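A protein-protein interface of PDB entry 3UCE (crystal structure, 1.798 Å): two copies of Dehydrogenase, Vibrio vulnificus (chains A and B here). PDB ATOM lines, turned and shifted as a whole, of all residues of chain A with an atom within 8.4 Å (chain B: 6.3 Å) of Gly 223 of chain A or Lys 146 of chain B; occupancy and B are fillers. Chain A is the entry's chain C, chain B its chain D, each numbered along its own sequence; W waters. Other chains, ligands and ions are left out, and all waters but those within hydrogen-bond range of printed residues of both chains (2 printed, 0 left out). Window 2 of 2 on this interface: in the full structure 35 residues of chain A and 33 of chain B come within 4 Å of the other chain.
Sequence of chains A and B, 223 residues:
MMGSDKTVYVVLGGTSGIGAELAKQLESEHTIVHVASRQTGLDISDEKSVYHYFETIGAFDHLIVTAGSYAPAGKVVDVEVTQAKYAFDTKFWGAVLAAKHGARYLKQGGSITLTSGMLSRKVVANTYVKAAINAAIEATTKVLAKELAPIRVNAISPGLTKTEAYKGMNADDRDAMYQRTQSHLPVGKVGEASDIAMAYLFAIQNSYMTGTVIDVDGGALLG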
ATOM      1  N   LYS A 122     -12.527  -0.512  -0.979  1.00  0.00           N
ATOM      2  CA  LYS A 122     -13.168  -1.562  -0.186  1.00  0.00           C
ATOM      3  C   LYS A 122     -13.271  -1.087   1.270  1.00  0.00           C
ATOM      4  O   LYS A 122     -12.265  -0.934   1.952  1.00  0.00           O
ATOM      5  CB  LYS A 122     -12.388  -2.877  -0.285  1.00  0.00           C
ATOM      6  CG  LYS A 122     -13.082  -4.088   0.357  1.00  0.00           C
ATOM      7  CD  LYS A 122     -12.172  -5.318   0.300  1.00  0.00           C
ATOM      8  CE  LYS A 122     -12.647  -6.456   1.214  1.00  0.00           C
ATOM      9  NZ  LYS A 122     -13.760  -7.231   0.616  1.00  0.00           N
ATOM     10  N   VAL A 123     -14.494  -0.840   1.730  1.00  0.00           N
ATOM     11  CA  VAL A 123     -14.718  -0.298   3.069  1.00  0.00           C
ATOM     12  C   VAL A 123     -14.580  -1.408   4.106  1.00  0.00           C
ATOM     13  O   VAL A 123     -15.387  -2.339   4.142  1.00  0.00           O
ATOM     14  CB  VAL A 123     -16.131   0.340   3.183  1.00  0.00           C
ATOM     15  CG1 VAL A 123     -16.267   1.160   4.464  1.00  0.00           C
ATOM     16  CG2 VAL A 123     -16.420   1.213   1.980  1.00  0.00           C
ATOM     17  N   HIS A 184     -11.351 -17.364   0.571  1.00  0.00           N
ATOM     18  CA  HIS A 184     -12.498 -16.498   0.299  1.00  0.00           C
ATOM     19  C   HIS A 184     -12.372 -15.595  -0.932  1.00  0.00           C
ATOM     20  O   HIS A 184     -13.355 -14.978  -1.333  1.00  0.00           O
ATOM     21  CB  HIS A 184     -12.819 -15.637   1.517  1.00  0.00           C
ATOM     22  CG  HIS A 184     -13.347 -16.418   2.679  1.00  0.00           C
ATOM     23  ND1 HIS A 184     -12.709 -17.534   3.180  1.00  0.00           N
ATOM     24  CD2 HIS A 184     -14.456 -16.245   3.438  1.00  0.00           C
ATOM     25  CE1 HIS A 184     -13.404 -18.015   4.196  1.00  0.00           C
ATOM     26  NE2 HIS A 184     -14.467 -17.252   4.373  1.00  0.00           N
ATOM     27  N   LEU A 185     -11.188 -15.499  -1.529  1.00  0.00           N
ATOM     28  CA  LEU A 185     -11.061 -14.697  -2.742  1.00  0.00           C
ATOM     29  C   LEU A 185     -11.605 -15.474  -3.936  1.00  0.00           C
ATOM     30  O   LEU A 185     -11.405 -16.695  -4.040  1.00  0.00           O
ATOM     31  CB  LEU A 185      -9.612 -14.276  -3.008  1.00  0.00           C
ATOM     32  CG  LEU A 185      -9.040 -13.186  -2.099  1.00  0.00           C
ATOM     33  CD1 LEU A 185      -7.623 -12.841  -2.539  1.00  0.00           C
ATOM     34  CD2 LEU A 185      -9.928 -11.931  -2.084  1.00  0.00           C
ATOM     35  N   PRO A 186     -12.320 -14.774  -4.833  1.00  0.00           N
ATOM     36  CA  PRO A 186     -12.759 -15.445  -6.058  1.00  0.00           C
ATOM     37  C   PRO A 186     -11.633 -16.212  -6.742  1.00  0.00           C
ATOM     38  O   PRO A 186     -11.879 -17.327  -7.199  1.00  0.00           O
ATOM     39  CB  PRO A 186     -13.254 -14.287  -6.929  1.00  0.00           C
ATOM     40  CG  PRO A 186     -13.802 -13.302  -5.926  1.00  0.00           C
ATOM     41  CD  PRO A 186     -12.905 -13.422  -4.701  1.00  0.00           C
ATOM     42  N   VAL A 187     -10.426 -15.655  -6.813  1.00  0.00           N
ATOM     43  CA  VAL A 187      -9.351 -16.350  -7.531  1.00  0.00           C
ATOM     44  C   VAL A 187      -8.782 -17.549  -6.767  1.00  0.00           C
ATOM     45  O   VAL A 187      -8.008 -18.329  -7.326  1.00  0.00           O
ATOM     46  CB  VAL A 187      -8.206 -15.411  -7.947  1.00  0.00           C
ATOM     47  CG1 VAL A 187      -8.716 -14.376  -8.950  1.00  0.00           C
ATOM     48  CG2 VAL A 187      -7.577 -14.739  -6.744  1.00  0.00           C
ATOM     49  N   ASP A 217      -6.304  -7.404  -7.318  1.00  0.00           N
ATOM     50  CA  ASP A 217      -6.701  -7.691  -5.941  1.00  0.00           C
ATOM     51  C   ASP A 217      -7.423  -9.024  -5.760  1.00  0.00           C
ATOM     52  O   ASP A 217      -8.089  -9.235  -4.743  1.00  0.00           O
ATOM     53  CB  ASP A 217      -7.590  -6.554  -5.414  1.00  0.00           C
ATOM     54  CG  ASP A 217      -9.036  -6.659  -5.885  1.00  0.00           C
ATOM     55  OD1 ASP A 217      -9.300  -7.301  -6.933  1.00  0.00           O
ATOM     56  OD2 ASP A 217      -9.917  -6.082  -5.197  1.00  0.00           O
ATOM     57  N   GLY A 218      -7.309  -9.912  -6.747  1.00  0.00           N
ATOM     58  CA  GLY A 218      -7.900 -11.245  -6.664  1.00  0.00           C
ATOM     59  C   GLY A 218      -9.413 -11.280  -6.489  1.00  0.00           C
ATOM     60  O   GLY A 218      -9.993 -12.326  -6.166  1.00  0.00           O
ATOM     61  N   GLY A 219     -10.057 -10.138  -6.698  1.00  0.00           N
ATOM     62  CA  GLY A 219     -11.494 -10.036  -6.555  1.00  0.00           C
ATOM     63  C   GLY A 219     -11.940  -9.471  -5.221  1.00  0.00           C
ATOM     64  O   GLY A 219     -13.133  -9.467  -4.926  1.00  0.00           O
ATOM     65  N   ALA A 220     -11.000  -8.996  -4.406  1.00  0.00           N
ATOM     66  CA  ALA A 220     -11.346  -8.510  -3.068  1.00  0.00           C
ATOM     67  C   ALA A 220     -12.424  -7.425  -3.129  1.00  0.00           C
ATOM     68  O   ALA A 220     -13.332  -7.395  -2.300  1.00  0.00           O
ATOM     69  CB  ALA A 220     -10.101  -7.991  -2.335  1.00  0.00           C
ATOM     70  N   LEU A 221     -12.333  -6.546  -4.122  1.00  0.00           N
ATOM     71  CA  LEU A 221     -13.287  -5.442  -4.251  1.00  0.00           C
ATOM     72  C   LEU A 221     -14.722  -5.905  -4.494  1.00  0.00           C
ATOM     73  O   LEU A 221     -15.663  -5.138  -4.294  1.00  0.00           O
ATOM     74  CB  LEU A 221     -12.858  -4.493  -5.375  1.00  0.00           C
ATOM     75  CG  LEU A 221     -11.712  -3.552  -5.003  1.00  0.00           C
ATOM     76  CD1 LEU A 221     -10.936  -3.122  -6.245  1.00  0.00           C
ATOM     77  CD2 LEU A 221     -12.238  -2.346  -4.236  1.00  0.00           C
ATOM     78  N   LEU A 222     -14.895  -7.151  -4.922  1.00  0.00           N
ATOM     79  CA  LEU A 222     -16.233  -7.676  -5.203  1.00  0.00           C
ATOM     80  C   LEU A 222     -17.027  -8.024  -3.936  1.00  0.00           C
ATOM     81  O   LEU A 222     -18.226  -8.314  -4.003  1.00  0.00           O
ATOM     82  CB  LEU A 222     -16.131  -8.911  -6.091  1.00  0.00           C
ATOM     83  CG  LEU A 222     -15.378  -8.674  -7.398  1.00  0.00           C
ATOM     84  CD1 LEU A 222     -15.235  -9.988  -8.170  1.00  0.00           C
ATOM     85  CD2 LEU A 222     -16.105  -7.623  -8.230  1.00  0.00           C
ATOM     86  N   GLY A 223     -16.360  -8.007  -2.788  1.00  0.00           N
ATOM     87  CA  GLY A 223     -17.034  -8.264  -1.529  1.00  0.00           C
ATOM     88  C   GLY A 223     -17.528  -9.696  -1.451  1.00  0.00           C
ATOM     89  O   GLY A 223     -17.033 -10.578  -2.155  1.00  0.00           O
ATOM     90  OXT GLY A 223     -18.432 -10.009  -0.678  1.00  0.00           O
ATOM     91  N   THR B 141     -19.890  -7.438 -15.840  1.00  0.00           N
ATOM     92  CA  THR B 141     -18.549  -8.003 -15.729  1.00  0.00           C
ATOM     93  C   THR B 141     -18.239  -8.361 -14.274  1.00  0.00           C
ATOM     94  O   THR B 141     -17.718  -9.443 -13.982  1.00  0.00           O
ATOM     95  CB  THR B 141     -17.478  -6.999 -16.192  1.00  0.00           C
ATOM     96  OG1 THR B 141     -17.609  -6.752 -17.596  1.00  0.00           O
ATOM     97  CG2 THR B 141     -16.072  -7.544 -15.901  1.00  0.00           C
ATOM     98  N   LYS B 142     -18.558  -7.451 -13.357  1.00  0.00           N
ATOM     99  CA  LYS B 142     -18.237  -7.682 -11.950  1.00  0.00           C
ATOM    100  C   LYS B 142     -19.124  -8.775 -11.336  1.00  0.00           C
ATOM    101  O   LYS B 142     -18.624  -9.630 -10.606  1.00  0.00           O
ATOM    102  CB  LYS B 142     -18.301  -6.374 -11.147  1.00  0.00           C
ATOM    103  CG  LYS B 142     -17.292  -5.344 -11.639  1.00  0.00           C
ATOM    104  CD  LYS B 142     -17.371  -4.010 -10.889  1.00  0.00           C
ATOM    105  CE  LYS B 142     -16.264  -3.057 -11.365  1.00  0.00           C
ATOM    106  NZ  LYS B 142     -16.092  -1.862 -10.492  1.00  0.00           N
ATOM    107  N   VAL B 143     -20.419  -8.762 -11.646  1.00  0.00           N
ATOM    108  CA  VAL B 143     -21.304  -9.845 -11.213  1.00  0.00           C
ATOM    109  C   VAL B 143     -20.820 -11.190 -11.741  1.00  0.00           C
ATOM    110  O   VAL B 143     -20.781 -12.172 -10.996  1.00  0.00           O
ATOM    111  CB  VAL B 143     -22.754  -9.614 -11.647  1.00  0.00           C
ATOM    112  CG1 VAL B 143     -23.627 -10.852 -11.333  1.00  0.00           C
ATOM    113  CG2 VAL B 143     -23.303  -8.380 -10.947  1.00  0.00           C
ATOM    114  N   LEU B 144     -20.446 -11.236 -13.017  1.00  0.00           N
ATOM    115  CA  LEU B 144     -19.892 -12.460 -13.607  1.00  0.00           C
ATOM    116  C   LEU B 144     -18.648 -12.930 -12.867  1.00  0.00           C
ATOM    117  O   LEU B 144     -18.471 -14.127 -12.633  1.00  0.00           O
ATOM    118  CB  LEU B 144     -19.536 -12.245 -15.079  1.00  0.00           C
ATOM    119  CG  LEU B 144     -20.697 -12.324 -16.066  1.00  0.00           C
ATOM    120  CD1 LEU B 144     -20.241 -11.837 -17.431  1.00  0.00           C
ATOM    121  CD2 LEU B 144     -21.244 -13.770 -16.147  1.00  0.00           C
ATOM    122  N   ALA B 145     -17.769 -11.996 -12.527  1.00  0.00           N
ATOM    123  CA  ALA B 145     -16.526 -12.350 -11.856  1.00  0.00           C
ATOM    124  C   ALA B 145     -16.837 -13.087 -10.550  1.00  0.00           C
ATOM    125  O   ALA B 145     -16.136 -14.009 -10.168  1.00  0.00           O
ATOM    126  CB  ALA B 145     -15.685 -11.096 -11.571  1.00  0.00           C
ATOM    127  N   LYS B 146     -17.904 -12.669  -9.880  1.00  0.00           N
ATOM    128  CA  LYS B 146     -18.298 -13.269  -8.614  1.00  0.00           C
ATOM    129  C   LYS B 146     -18.962 -14.637  -8.823  1.00  0.00           C
ATOM    130  O   LYS B 146     -18.687 -15.599  -8.095  1.00  0.00           O
ATOM    131  CB  LYS B 146     -19.255 -12.319  -7.901  1.00  0.00           C
ATOM    132  CG  LYS B 146     -19.434 -12.593  -6.449  1.00  0.00           C
ATOM    133  CD  LYS B 146     -19.998 -11.376  -5.757  1.00  0.00           C
ATOM    134  CE  LYS B 146     -19.434 -11.240  -4.359  1.00  0.00           C
ATOM    135  NZ  LYS B 146     -20.307 -10.355  -3.554  1.00  0.00           N
ATOM    136  N   GLU B 147     -19.820 -14.722  -9.835  1.00  0.00           N
ATOM    137  CA  GLU B 147     -20.564 -15.948 -10.109  1.00  0.00           C
ATOM    138  C   GLU B 147     -19.712 -17.069 -10.699  1.00  0.00           C
ATOM    139  O   GLU B 147     -19.945 -18.241 -10.404  1.00  0.00           O
ATOM    140  CB  GLU B 147     -21.742 -15.652 -11.042  1.00  0.00           C
ATOM    141  CG  GLU B 147     -22.827 -14.862 -10.350  1.00  0.00           C
ATOM    142  CD  GLU B 147     -23.931 -14.406 -11.275  1.00  0.00           C
ATOM    143  OE1 GLU B 147     -23.870 -14.699 -12.495  1.00  0.00           O
ATOM    144  OE2 GLU B 147     -24.874 -13.765 -10.759  1.00  0.00           O
ATOM    145  N   LEU B 148     -18.740 -16.726 -11.535  1.00  0.00           N
ATOM    146  CA  LEU B 148     -18.005 -17.745 -12.282  1.00  0.00           C
ATOM    147  C   LEU B 148     -16.700 -18.166 -11.619  1.00  0.00           C
ATOM    148  O   LEU B 148     -16.062 -19.113 -12.083  1.00  0.00           O
ATOM    149  CB  LEU B 148     -17.711 -17.278 -13.717  1.00  0.00           C
ATOM    150  CG  LEU B 148     -18.894 -17.010 -14.657  1.00  0.00           C
ATOM    151  CD1 LEU B 148     -18.382 -16.681 -16.055  1.00  0.00           C
ATOM    152  CD2 LEU B 148     -19.873 -18.183 -14.712  1.00  0.00           C
ATOM    153  N   ALA B 149     -16.295 -17.469 -10.554  1.00  0.00           N
ATOM    154  CA  ALA B 149     -15.046 -17.780  -9.858  1.00  0.00           C
ATOM    155  C   ALA B 149     -14.938 -19.287  -9.631  1.00  0.00           C
ATOM    156  O   ALA B 149     -15.937 -19.936  -9.305  1.00  0.00           O
ATOM    157  CB  ALA B 149     -14.978 -17.029  -8.529  1.00  0.00           C
ATOM    158  N   ILE B 151     -13.122 -18.965 -12.368  1.00  0.00           N
ATOM    159  CA  ILE B 151     -12.946 -18.397 -13.696  1.00  0.00           C
ATOM    160  C   ILE B 151     -12.902 -16.886 -13.508  1.00  0.00           C
ATOM    161  O   ILE B 151     -13.742 -16.320 -12.800  1.00  0.00           O
ATOM    162  CB  ILE B 151     -14.083 -18.755 -14.652  1.00  0.00           C
ATOM    163  CG1 ILE B 151     -14.056 -20.250 -14.968  1.00  0.00           C
ATOM    164  CG2 ILE B 151     -13.945 -17.947 -15.938  1.00  0.00           C
ATOM    165  CD1 ILE B 151     -12.751 -20.705 -15.602  1.00  0.00           C
ATOM    166  N   VAL B 153     -13.041 -12.881 -14.621  1.00  0.00           N
ATOM    167  CA  VAL B 153     -13.799 -12.080 -15.579  1.00  0.00           C
ATOM    168  C   VAL B 153     -13.445 -10.610 -15.405  1.00  0.00           C
ATOM    169  O   VAL B 153     -13.589 -10.056 -14.320  1.00  0.00           O
ATOM    170  CB  VAL B 153     -15.305 -12.260 -15.424  1.00  0.00           C
ATOM    171  CG1 VAL B 153     -16.037 -11.552 -16.575  1.00  0.00           C
ATOM    172  CG2 VAL B 153     -15.658 -13.744 -15.412  1.00  0.00           C
ATOM    173  N   THR B 210      -9.411 -10.225 -11.194  1.00  0.00           N
ATOM    174  CA  THR B 210     -10.756 -10.531 -11.629  1.00  0.00           C
ATOM    175  C   THR B 210     -11.687  -9.445 -11.126  1.00  0.00           C
ATOM    176  O   THR B 210     -11.442  -8.865 -10.071  1.00  0.00           O
ATOM    177  CB  THR B 210     -11.226 -11.916 -11.120  1.00  0.00           C
ATOM    178  OG1 THR B 210     -12.423 -12.291 -11.805  1.00  0.00           O
ATOM    179  CG2 THR B 210     -11.476 -11.920  -9.596  1.00  0.00           C
HETATM  180  O   HOH W   1     -11.835  -6.911  -7.903  1.00  0.00           O
HETATM  181  O   HOH W   2      -8.501  -7.735  -9.584  1.00  0.00           O
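The side-chain amino group (NZ) of Lys 146 of chain B sits at hydrogen-bond distance from the backbone carbonyl oxygen (O) of Leu 222 of chain A. The side-chain amino group (NZ) of Lys 146 of chain B is in salt-bridge range of the chain-end carboxylate (OXT) of Gly 223 of chain A, 3.5 Å away.
Water W1 lies within hydrogen-bond range of OD1 of Asp 217 of chain A and O of Thr 210 of chain B. Water W2 bridges the side-chain carboxylate (OD1) of Asp 217 of chain A (2.8 Å) and the backbone NH (N) of Thr 210 of chain B (3.1 Å).
No position is printed for both chains.
Hydrophobic or aromatic side chains of chain A within 4 Å of the printed part of chain B: Pro 186, Val 187 and Leu 222. Of the 12 printed residues of chain B, 5 touch a printed residue of chain A. Among the printed residues, 9 pairs touch across the chains.
The backbone NH of Val 187 of chain A lies within hydrogen-bond range of the backbone carbonyl oxygen of Gly 218 of chain A (3.4 Å). N of Gly 219 of chain A lies within hydrogen-bond range of OD1 of Asp 217 of chain A (2.9 Å). N of Val 153 of chain B is in hydrogen-bond range of OG1 of Thr 210 of chain B, at 2.9 Å.
Among the printed residues, merely in contact across the chains: Pro 186 of chain A with Ala 149 of chain B, Pro 186 of chain A with Thr 210 of chain B, Val 187 of chain A with Thr 210 of chain B, Gly 218 of chain A with Thr 210 of chain B, Gly 219 of chain A with Thr 210 of chain B, Leu 222 of chain A with Lys 142 of chain B and Leu 222 of chain A with Ala 145 of chain B.
Of chain B, only Lys 146 comes within 4 Å of Gly 223 of chain A. Of chain A, only Leu 222 (2.9 Å) and Gly 223 (3.3 Å) come within 4 Å of Lys 146 of chain B. Ala 145 of chain B touches just one residue of chain A: Leu 222. Of the printed residues of chain B, Gly 219 of chain A touches Thr 210 (3.6 Å). Printed residues of chain B within 4 Å of Gly 218 of chain A: Thr 210 (3.8 Å). Of the printed residues of chain A, Thr 210 of chain B touches Pro 186, Val 187, Gly 218 and Gly 219. Printed residues of chain B within 4 Å of Pro 186 of chain A: Ala 149 and Thr 210. Of the printed residues of chain A, Lys 142 of chain B touches Leu 222 (3.9 Å). Ala 220 of chain A touches none of the printed residues of chain B. Leu 148 of chain B touches none of the printed residues of chain A. The nearest printed residue of chain B that does not touch Gly 223 of chain A is Lys 142 of chain B (8.3 Å).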
